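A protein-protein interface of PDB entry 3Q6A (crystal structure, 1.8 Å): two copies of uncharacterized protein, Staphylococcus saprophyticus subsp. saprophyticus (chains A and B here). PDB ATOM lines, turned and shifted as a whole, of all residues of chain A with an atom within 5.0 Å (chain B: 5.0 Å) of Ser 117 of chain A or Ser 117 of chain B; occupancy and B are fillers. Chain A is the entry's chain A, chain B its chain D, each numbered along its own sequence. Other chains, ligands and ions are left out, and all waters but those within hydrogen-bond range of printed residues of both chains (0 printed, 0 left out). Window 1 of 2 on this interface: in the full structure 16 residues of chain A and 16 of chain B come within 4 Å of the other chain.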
ATOM      1  N   MET A   7     -30.616   4.169 -17.739  1.00  0.00           N
ATOM      2  CA  MET A   7     -30.237   2.794 -18.077  1.00  0.00           C
ATOM      3  C   MET A   7     -31.275   2.163 -18.988  1.00  0.00           C
ATOM      4  O   MET A   7     -32.479   2.250 -18.726  1.00  0.00           O
ATOM      5  CB  MET A   7     -30.127   1.936 -16.803  1.00  0.00           C
ATOM      6  CG  MET A   7     -29.739   0.484 -17.055  1.00  0.00           C
ATOM      7  SD  MET A   7     -28.005   0.313 -17.454  1.00  0.00           S
ATOM      8  CE  MET A   7     -27.432  -0.007 -15.933  1.00  0.00           C
ATOM      9  N   TRP A 112     -26.592   4.657  -7.719  1.00  0.00           N
ATOM     10  CA  TRP A 112     -27.640   4.578  -8.739  1.00  0.00           C
ATOM     11  C   TRP A 112     -27.232   3.703  -9.905  1.00  0.00           C
ATOM     12  O   TRP A 112     -28.036   2.908 -10.385  1.00  0.00           O
ATOM     13  CB  TRP A 112     -28.027   5.970  -9.269  1.00  0.00           C
ATOM     14  CG  TRP A 112     -28.719   6.781  -8.221  1.00  0.00           C
ATOM     15  CD1 TRP A 112     -28.185   7.798  -7.482  1.00  0.00           C
ATOM     16  CD2 TRP A 112     -30.038   6.567  -7.720  1.00  0.00           C
ATOM     17  NE1 TRP A 112     -29.095   8.229  -6.542  1.00  0.00           N
ATOM     18  CE2 TRP A 112     -30.243   7.491  -6.661  1.00  0.00           C
ATOM     19  CE3 TRP A 112     -31.080   5.684  -8.058  1.00  0.00           C
ATOM     20  CZ2 TRP A 112     -31.443   7.551  -5.933  1.00  0.00           C
ATOM     21  CZ3 TRP A 112     -32.278   5.746  -7.329  1.00  0.00           C
ATOM     22  CH2 TRP A 112     -32.443   6.674  -6.278  1.00  0.00           C
ATOM     23  N   VAL A 113     -25.986   3.835 -10.350  1.00  0.00           N
ATOM     24  CA  VAL A 113     -25.531   3.034 -11.491  1.00  0.00           C
ATOM     25  C   VAL A 113     -25.568   1.546 -11.168  1.00  0.00           C
ATOM     26  O   VAL A 113     -26.012   0.722 -11.994  1.00  0.00           O
ATOM     27  CB  VAL A 113     -24.116   3.455 -11.929  1.00  0.00           C
ATOM     28  CG1 VAL A 113     -23.615   2.507 -13.029  1.00  0.00           C
ATOM     29  CG2 VAL A 113     -24.136   4.886 -12.442  1.00  0.00           C
ATOM     30  N   TYR A 114     -25.091   1.192  -9.981  1.00  0.00           N
ATOM     31  CA  TYR A 114     -25.096  -0.204  -9.554  1.00  0.00           C
ATOM     32  C   TYR A 114     -26.517  -0.750  -9.425  1.00  0.00           C
ATOM     33  O   TYR A 114     -26.808  -1.848  -9.912  1.00  0.00           O
ATOM     34  CB  TYR A 114     -24.371  -0.375  -8.217  1.00  0.00           C
ATOM     35  CG  TYR A 114     -24.279  -1.822  -7.788  1.00  0.00           C
ATOM     36  CD1 TYR A 114     -23.539  -2.738  -8.528  1.00  0.00           C
ATOM     37  CD2 TYR A 114     -24.943  -2.273  -6.650  1.00  0.00           C
ATOM     38  CE1 TYR A 114     -23.462  -4.077  -8.147  1.00  0.00           C
ATOM     39  CE2 TYR A 114     -24.875  -3.609  -6.251  1.00  0.00           C
ATOM     40  CZ  TYR A 114     -24.129  -4.511  -7.012  1.00  0.00           C
ATOM     41  OH  TYR A 114     -24.065  -5.840  -6.650  1.00  0.00           O
ATOM     42  N   MET A 115     -27.410   0.000  -8.784  1.00  0.00           N
ATOM     43  CA  MET A 115     -28.799  -0.465  -8.649  1.00  0.00           C
ATOM     44  C   MET A 115     -29.442  -0.703 -10.020  1.00  0.00           C
ATOM     45  O   MET A 115     -30.144  -1.696 -10.226  1.00  0.00           O
ATOM     46  CB  MET A 115     -29.644   0.560  -7.876  1.00  0.00           C
ATOM     47  CG  MET A 115     -31.111   0.133  -7.614  1.00  0.00           C
ATOM     48  SD  MET A 115     -32.311   0.379  -8.993  1.00  0.00           S
ATOM     49  CE  MET A 115     -32.642   2.199  -8.789  1.00  0.00           C
ATOM     50  N   LEU A 116     -29.209   0.205 -10.961  1.00  0.00           N
ATOM     51  CA  LEU A 116     -29.813   0.045 -12.279  1.00  0.00           C
ATOM     52  C   LEU A 116     -29.223  -1.150 -13.015  1.00  0.00           C
ATOM     53  O   LEU A 116     -29.914  -1.786 -13.804  1.00  0.00           O
ATOM     54  CB  LEU A 116     -29.671   1.322 -13.109  1.00  0.00           C
ATOM     55  CG  LEU A 116     -30.489   2.496 -12.539  1.00  0.00           C
ATOM     56  CD1 LEU A 116     -30.074   3.762 -13.259  1.00  0.00           C
ATOM     57  CD2 LEU A 116     -32.011   2.253 -12.679  1.00  0.00           C
ATOM     58  N   SER A 117     -27.946  -1.441 -12.758  1.00  0.00           N
ATOM     59  CA  SER A 117     -27.289  -2.589 -13.361  1.00  0.00           C
ATOM     60  C   SER A 117     -27.894  -3.863 -12.777  1.00  0.00           C
ATOM     61  O   SER A 117     -28.112  -4.840 -13.485  1.00  0.00           O
ATOM     62  CB  SER A 117     -25.779  -2.539 -13.070  1.00  0.00           C
ATOM     63  OG  SER A 117     -25.188  -1.419 -13.699  1.00  0.00           O
ATOM     64  N   CYS A 118     -28.139  -3.866 -11.469  1.00  0.00           N
ATOM     65  CA  CYS A 118     -28.753  -5.027 -10.833  1.00  0.00           C
ATOM     66  C   CYS A 118     -30.150  -5.223 -11.424  1.00  0.00           C
ATOM     67  O   CYS A 118     -30.579  -6.352 -11.668  1.00  0.00           O
ATOM     68  CB  CYS A 118     -28.871  -4.829  -9.319  1.00  0.00           C
ATOM     69  SG  CYS A 118     -27.291  -4.841  -8.409  1.00  0.00           S
ATOM     70  N   LEU A 119     -30.854  -4.115 -11.657  1.00  0.00           N
ATOM     71  CA  LEU A 119     -32.195  -4.166 -12.234  1.00  0.00           C
ATOM     72  C   LEU A 119     -32.157  -4.785 -13.638  1.00  0.00           C
ATOM     73  O   LEU A 119     -32.977  -5.638 -13.987  1.00  0.00           O
ATOM     74  CB  LEU A 119     -32.774  -2.752 -12.344  1.00  0.00           C
ATOM     75  CG  LEU A 119     -34.090  -2.605 -13.117  1.00  0.00           C
ATOM     76  CD1 LEU A 119     -35.248  -3.199 -12.312  1.00  0.00           C
ATOM     77  CD2 LEU A 119     -34.341  -1.135 -13.382  1.00  0.00           C
ATOM     78  N   LYS A 120     -31.214  -4.320 -14.447  1.00  0.00           N
ATOM     79  CA  LYS A 120     -31.076  -4.823 -15.816  1.00  0.00           C
ATOM     80  C   LYS A 120     -30.889  -6.355 -15.878  1.00  0.00           C
ATOM     81  O   LYS A 120     -31.597  -7.043 -16.629  1.00  0.00           O
ATOM     82  CB  LYS A 120     -29.911  -4.104 -16.500  1.00  0.00           C
ATOM     83  CG  LYS A 120     -29.855  -4.297 -18.010  1.00  0.00           C
ATOM     84  CD  LYS A 120     -28.720  -3.499 -18.614  1.00  0.00           C
ATOM     85  CE  LYS A 120     -28.517  -3.826 -20.094  1.00  0.00           C
ATOM     86  NZ  LYS A 120     -29.712  -3.558 -20.936  1.00  0.00           N
ATOM     87  N   VAL A 121     -29.964  -6.893 -15.085  1.00  0.00           N
ATOM     88  CA  VAL A 121     -29.709  -8.351 -15.076  1.00  0.00           C
ATOM     89  C   VAL A 121     -30.920  -9.112 -14.559  1.00  0.00           C
ATOM     90  O   VAL A 121     -31.346 -10.106 -15.136  1.00  0.00           O
ATOM     91  CB  VAL A 121     -28.507  -8.706 -14.181  1.00  0.00           C
ATOM     92  CG1 VAL A 121     -28.149 -10.177 -14.349  1.00  0.00           C
ATOM     93  CG2 VAL A 121     -27.333  -7.818 -14.543  1.00  0.00           C
ATOM     94  N   ILE A 129     -27.498 -10.181  -8.841  1.00  0.00           N
ATOM     95  CA  ILE A 129     -26.194  -9.936  -8.257  1.00  0.00           C
ATOM     96  C   ILE A 129     -26.505  -9.165  -6.964  1.00  0.00           C
ATOM     97  O   ILE A 129     -27.487  -8.435  -6.901  1.00  0.00           O
ATOM     98  CB  ILE A 129     -25.265  -9.122  -9.185  1.00  0.00           C
ATOM     99  CG1 ILE A 129     -26.002  -7.921  -9.780  1.00  0.00           C
ATOM    100  CG2 ILE A 129     -24.729 -10.031 -10.286  1.00  0.00           C
ATOM    101  CD1 ILE A 129     -25.080  -6.943 -10.463  1.00  0.00           C
ATOM    102  N   MET B   7     -15.324  -3.482  -6.686  1.00  0.00           N
ATOM    103  CA  MET B   7     -16.444  -4.384  -6.950  1.00  0.00           C
ATOM    104  C   MET B   7     -16.106  -5.813  -6.539  1.00  0.00           C
ATOM    105  O   MET B   7     -15.077  -6.354  -6.933  1.00  0.00           O
ATOM    106  CB  MET B   7     -16.804  -4.386  -8.435  1.00  0.00           C
ATOM    107  CG  MET B   7     -17.998  -5.285  -8.787  1.00  0.00           C
ATOM    108  SD  MET B   7     -19.595  -4.638  -8.180  1.00  0.00           S
ATOM    109  CE  MET B   7     -19.853  -3.225  -9.387  1.00  0.00           C
ATOM    110  N   TRP B 112     -16.949   3.241 -14.969  1.00  0.00           N
ATOM    111  CA  TRP B 112     -16.238   2.241 -14.175  1.00  0.00           C
ATOM    112  C   TRP B 112     -17.204   1.363 -13.416  1.00  0.00           C
ATOM    113  O   TRP B 112     -17.044   0.145 -13.401  1.00  0.00           O
ATOM    114  CB  TRP B 112     -15.280   2.916 -13.194  1.00  0.00           C
ATOM    115  CG  TRP B 112     -14.065   3.493 -13.862  1.00  0.00           C
ATOM    116  CD1 TRP B 112     -13.742   4.820 -13.984  1.00  0.00           C
ATOM    117  CD2 TRP B 112     -13.037   2.762 -14.545  1.00  0.00           C
ATOM    118  NE1 TRP B 112     -12.575   4.958 -14.709  1.00  0.00           N
ATOM    119  CE2 TRP B 112     -12.124   3.710 -15.065  1.00  0.00           C
ATOM    120  CE3 TRP B 112     -12.800   1.393 -14.772  1.00  0.00           C
ATOM    121  CZ2 TRP B 112     -10.992   3.334 -15.796  1.00  0.00           C
ATOM    122  CZ3 TRP B 112     -11.674   1.023 -15.500  1.00  0.00           C
ATOM    123  CH2 TRP B 112     -10.785   1.991 -16.003  1.00  0.00           C
ATOM    124  N   VAL B 113     -18.225   1.970 -12.812  1.00  0.00           N
ATOM    125  CA  VAL B 113     -19.198   1.176 -12.061  1.00  0.00           C
ATOM    126  C   VAL B 113     -19.958   0.246 -12.984  1.00  0.00           C
ATOM    127  O   VAL B 113     -20.159  -0.912 -12.666  1.00  0.00           O
ATOM    128  CB  VAL B 113     -20.213   2.063 -11.324  1.00  0.00           C
ATOM    129  CG1 VAL B 113     -21.228   1.184 -10.587  1.00  0.00           C
ATOM    130  CG2 VAL B 113     -19.472   2.973 -10.333  1.00  0.00           C
ATOM    131  N   TYR B 114     -20.396   0.762 -14.127  1.00  0.00           N
ATOM    132  CA  TYR B 114     -21.120  -0.080 -15.071  1.00  0.00           C
ATOM    133  C   TYR B 114     -20.246  -1.248 -15.574  1.00  0.00           C
ATOM    134  O   TYR B 114     -20.675  -2.395 -15.574  1.00  0.00           O
ATOM    135  CB  TYR B 114     -21.596   0.756 -16.262  1.00  0.00           C
ATOM    136  CG  TYR B 114     -22.462  -0.027 -17.208  1.00  0.00           C
ATOM    137  CD1 TYR B 114     -23.645  -0.619 -16.770  1.00  0.00           C
ATOM    138  CD2 TYR B 114     -22.087  -0.211 -18.539  1.00  0.00           C
ATOM    139  CE1 TYR B 114     -24.440  -1.384 -17.641  1.00  0.00           C
ATOM    140  CE2 TYR B 114     -22.877  -0.974 -19.417  1.00  0.00           C
ATOM    141  CZ  TYR B 114     -24.046  -1.554 -18.960  1.00  0.00           C
ATOM    142  OH  TYR B 114     -24.834  -2.286 -19.829  1.00  0.00           O
ATOM    143  N   MET B 115     -19.024  -0.957 -16.020  1.00  0.00           N
ATOM    144  CA  MET B 115     -18.167  -2.038 -16.515  1.00  0.00           C
ATOM    145  C   MET B 115     -17.968  -3.137 -15.463  1.00  0.00           C
ATOM    146  O   MET B 115     -18.031  -4.325 -15.784  1.00  0.00           O
ATOM    147  CB  MET B 115     -16.793  -1.495 -16.958  1.00  0.00           C
ATOM    148  CG  MET B 115     -15.802  -2.570 -17.526  1.00  0.00           C
ATOM    149  SD  MET B 115     -14.825  -3.513 -16.283  1.00  0.00           S
ATOM    150  CE  MET B 115     -13.665  -2.295 -15.845  1.00  0.00           C
ATOM    151  N   LEU B 116     -17.746  -2.738 -14.218  1.00  0.00           N
ATOM    152  CA  LEU B 116     -17.510  -3.699 -13.135  1.00  0.00           C
ATOM    153  C   LEU B 116     -18.786  -4.481 -12.832  1.00  0.00           C
ATOM    154  O   LEU B 116     -18.727  -5.639 -12.402  1.00  0.00           O
ATOM    155  CB  LEU B 116     -16.971  -2.966 -11.881  1.00  0.00           C
ATOM    156  CG  LEU B 116     -15.533  -2.430 -12.035  1.00  0.00           C
ATOM    157  CD1 LEU B 116     -15.137  -1.544 -10.857  1.00  0.00           C
ATOM    158  CD2 LEU B 116     -14.578  -3.627 -12.159  1.00  0.00           C
ATOM    159  N   SER B 117     -19.948  -3.860 -13.059  1.00  0.00           N
ATOM    160  CA  SER B 117     -21.224  -4.551 -12.840  1.00  0.00           C
ATOM    161  C   SER B 117     -21.404  -5.580 -13.935  1.00  0.00           C
ATOM    162  O   SER B 117     -21.862  -6.687 -13.684  1.00  0.00           O
ATOM    163  CB  SER B 117     -22.406  -3.563 -12.870  1.00  0.00           C
ATOM    164  OG  SER B 117     -22.286  -2.656 -11.795  1.00  0.00           O
ATOM    165  N   CYS B 118     -21.053  -5.209 -15.161  1.00  0.00           N
ATOM    166  CA  CYS B 118     -21.139  -6.136 -16.284  1.00  0.00           C
ATOM    167  C   CYS B 118     -20.153  -7.278 -16.017  1.00  0.00           C
ATOM    168  O   CYS B 118     -20.440  -8.437 -16.302  1.00  0.00           O
ATOM    169  CB  CYS B 118     -20.753  -5.437 -17.580  1.00  0.00           C
ATOM    170  SG  CYS B 118     -21.940  -4.191 -18.119  1.00  0.00           S
ATOM    171  N   LEU B 119     -18.985  -6.932 -15.487  1.00  0.00           N
ATOM    172  CA  LEU B 119     -17.972  -7.938 -15.166  1.00  0.00           C
ATOM    173  C   LEU B 119     -18.543  -8.968 -14.180  1.00  0.00           C
ATOM    174  O   LEU B 119     -18.478 -10.182 -14.416  1.00  0.00           O
ATOM    175  CB  LEU B 119     -16.748  -7.266 -14.555  1.00  0.00           C
ATOM    176  CG  LEU B 119     -15.678  -8.219 -14.020  1.00  0.00           C
ATOM    177  CD1 LEU B 119     -15.062  -8.997 -15.189  1.00  0.00           C
ATOM    178  CD2 LEU B 119     -14.647  -7.454 -13.233  1.00  0.00           C
ATOM    179  N   LYS B 120     -19.112  -8.469 -13.089  1.00  0.00           N
ATOM    180  CA  LYS B 120     -19.676  -9.309 -12.032  1.00  0.00           C
ATOM    181  C   LYS B 120     -20.740 -10.266 -12.563  1.00  0.00           C
ATOM    182  O   LYS B 120     -20.737 -11.476 -12.253  1.00  0.00           O
ATOM    183  CB  LYS B 120     -20.239  -8.414 -10.924  1.00  0.00           C
ATOM    184  CG  LYS B 120     -20.815  -9.162  -9.712  1.00  0.00           C
ATOM    185  CD  LYS B 120     -21.414  -8.202  -8.695  1.00  0.00           C
ATOM    186  CE  LYS B 120     -21.997  -8.941  -7.478  1.00  0.00           C
ATOM    187  NZ  LYS B 120     -20.935  -9.602  -6.619  1.00  0.00           N
ATOM    188  N   VAL B 121     -21.642  -9.739 -13.385  1.00  0.00           N
ATOM    189  CA  VAL B 121     -22.694 -10.562 -13.956  1.00  0.00           C
ATOM    190  C   VAL B 121     -22.141 -11.632 -14.900  1.00  0.00           C
ATOM    191  O   VAL B 121     -22.583 -12.783 -14.877  1.00  0.00           O
ATOM    192  CB  VAL B 121     -23.694  -9.709 -14.745  1.00  0.00           C
ATOM    193  CG1 VAL B 121     -24.750 -10.603 -15.374  1.00  0.00           C
ATOM    194  CG2 VAL B 121     -24.328  -8.679 -13.816  1.00  0.00           C
ATOM    195  N   ILE B 129     -24.849  -8.155 -19.910  1.00  0.00           N
ATOM    196  CA  ILE B 129     -25.819  -7.066 -19.926  1.00  0.00           C
ATOM    197  C   ILE B 129     -25.293  -5.853 -20.670  1.00  0.00           C
ATOM    198  O   ILE B 129     -24.990  -4.822 -20.053  1.00  0.00           O
ATOM    199  CB  ILE B 129     -26.209  -6.617 -18.509  1.00  0.00           C
ATOM    200  CG1 ILE B 129     -24.953  -6.489 -17.640  1.00  0.00           C
ATOM    201  CG2 ILE B 129     -27.224  -7.577 -17.936  1.00  0.00           C
ATOM    202  CD1 ILE B 129     -25.136  -5.632 -16.376  1.00  0.00           C
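Among the printed residues, merely in contact across the chains: Val 121 of chain A with Val 121 of chain B (3.2 Å), Val 121 of chain A with Ile 129 of chain B (3.4 Å), Tyr 114 of chain A with Ser 117 of chain B (3.5 Å), Ser 117 of chain A with Tyr 114 of chain B (3.5 Å), Ser 117 of chain A with Ser 117 of chain B (3.5 Å), Val 113 of chain A with Val 113 of chain B (3.7 Å), Lys 120 of chain A with Ile 129 of chain B (3.7 Å), Ile 129 of chain A with Lys 120 of chain B (3.7 Å), Met 7 of chain A with Tyr 114 of chain B (3.7 Å), Ile 129 of chain A with Val 121 of chain B (3.8 Å), Tyr 114 of chain A with Met 7 of chain B (3.8 Å), Tyr 114 of chain A with Lys 120 of chain B (3.8 Å), Val 113 of chain A with Tyr 114 of chain B (3.8 Å) and Tyr 114 of chain A with Val 113 of chain B (3.9 Å).
OG of Ser 117 of chain B lies within hydrogen-bond range of O of Val 113 of chain B, 2.9 Å away. O of Val 113 of chain A lies within hydrogen-bond range of OG of Ser 117 of chain A (2.9 Å). SG of Cys 118 of chain B sits at hydrogen-bond distance from O of Tyr 114 of chain B. OH of Tyr 114 of chain B lies within hydrogen-bond range of O of Ile 129 of chain B, at 2.6 Å. SG of Cys 118 of chain B lies within hydrogen-bond range of O of Ile 129 of chain B (3.7 Å). O of Tyr 114 of chain A lies within hydrogen-bond range of SG of Cys 118 of chain A, 3.4 Å away.
Met 7 of chain A touches Tyr 114 of chain B, and with the chains exchanged Tyr 114 of chain A touches Met 7 of chain B. Val 113 of chain B touches its own counterpart, Val 113 of chain A. Tyr 114 of chain A touches Lys 120 of chain B, but with the chains exchanged Lys 120 of chain A does not touch Tyr 114 of chain B (4.001 Å). Lys 120 of chain A touches Ile 129 of chain B, and with the chains exchanged Ile 129 of chain A touches Lys 120 of chain B.
Ser 117 of chain A touches just these residues of chain B: Tyr 114 (3.5 Å) and Ser 117 (3.5 Å). Ser 117 of chain B touches just these residues of chain A: Tyr 114 (3.5 Å) and Ser 117 (3.5 Å). Of the printed residues of chain A, Tyr 114 of chain B touches Met 7, Val 113 and Ser 117. Of the printed residues of chain A, Met 7 of chain B touches Tyr 114 (3.8 Å). Printed residues of chain A within 4 Å of Val 113 of chain B: Val 113 (3.7 Å) and Tyr 114 (3.9 Å). The nearest residue of chain A that does not touch Ser 117 of chain B is Ile 129 of chain A (4.6 Å). The nearest printed residue of chain B that does not touch Met 7 of chain A is Ile 129 of chain B (6.1 Å).
Of the 12 printed residues of chain A, 7 touch a printed residue of chain B. Among the printed residues, 14 pairs touch across the chains.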
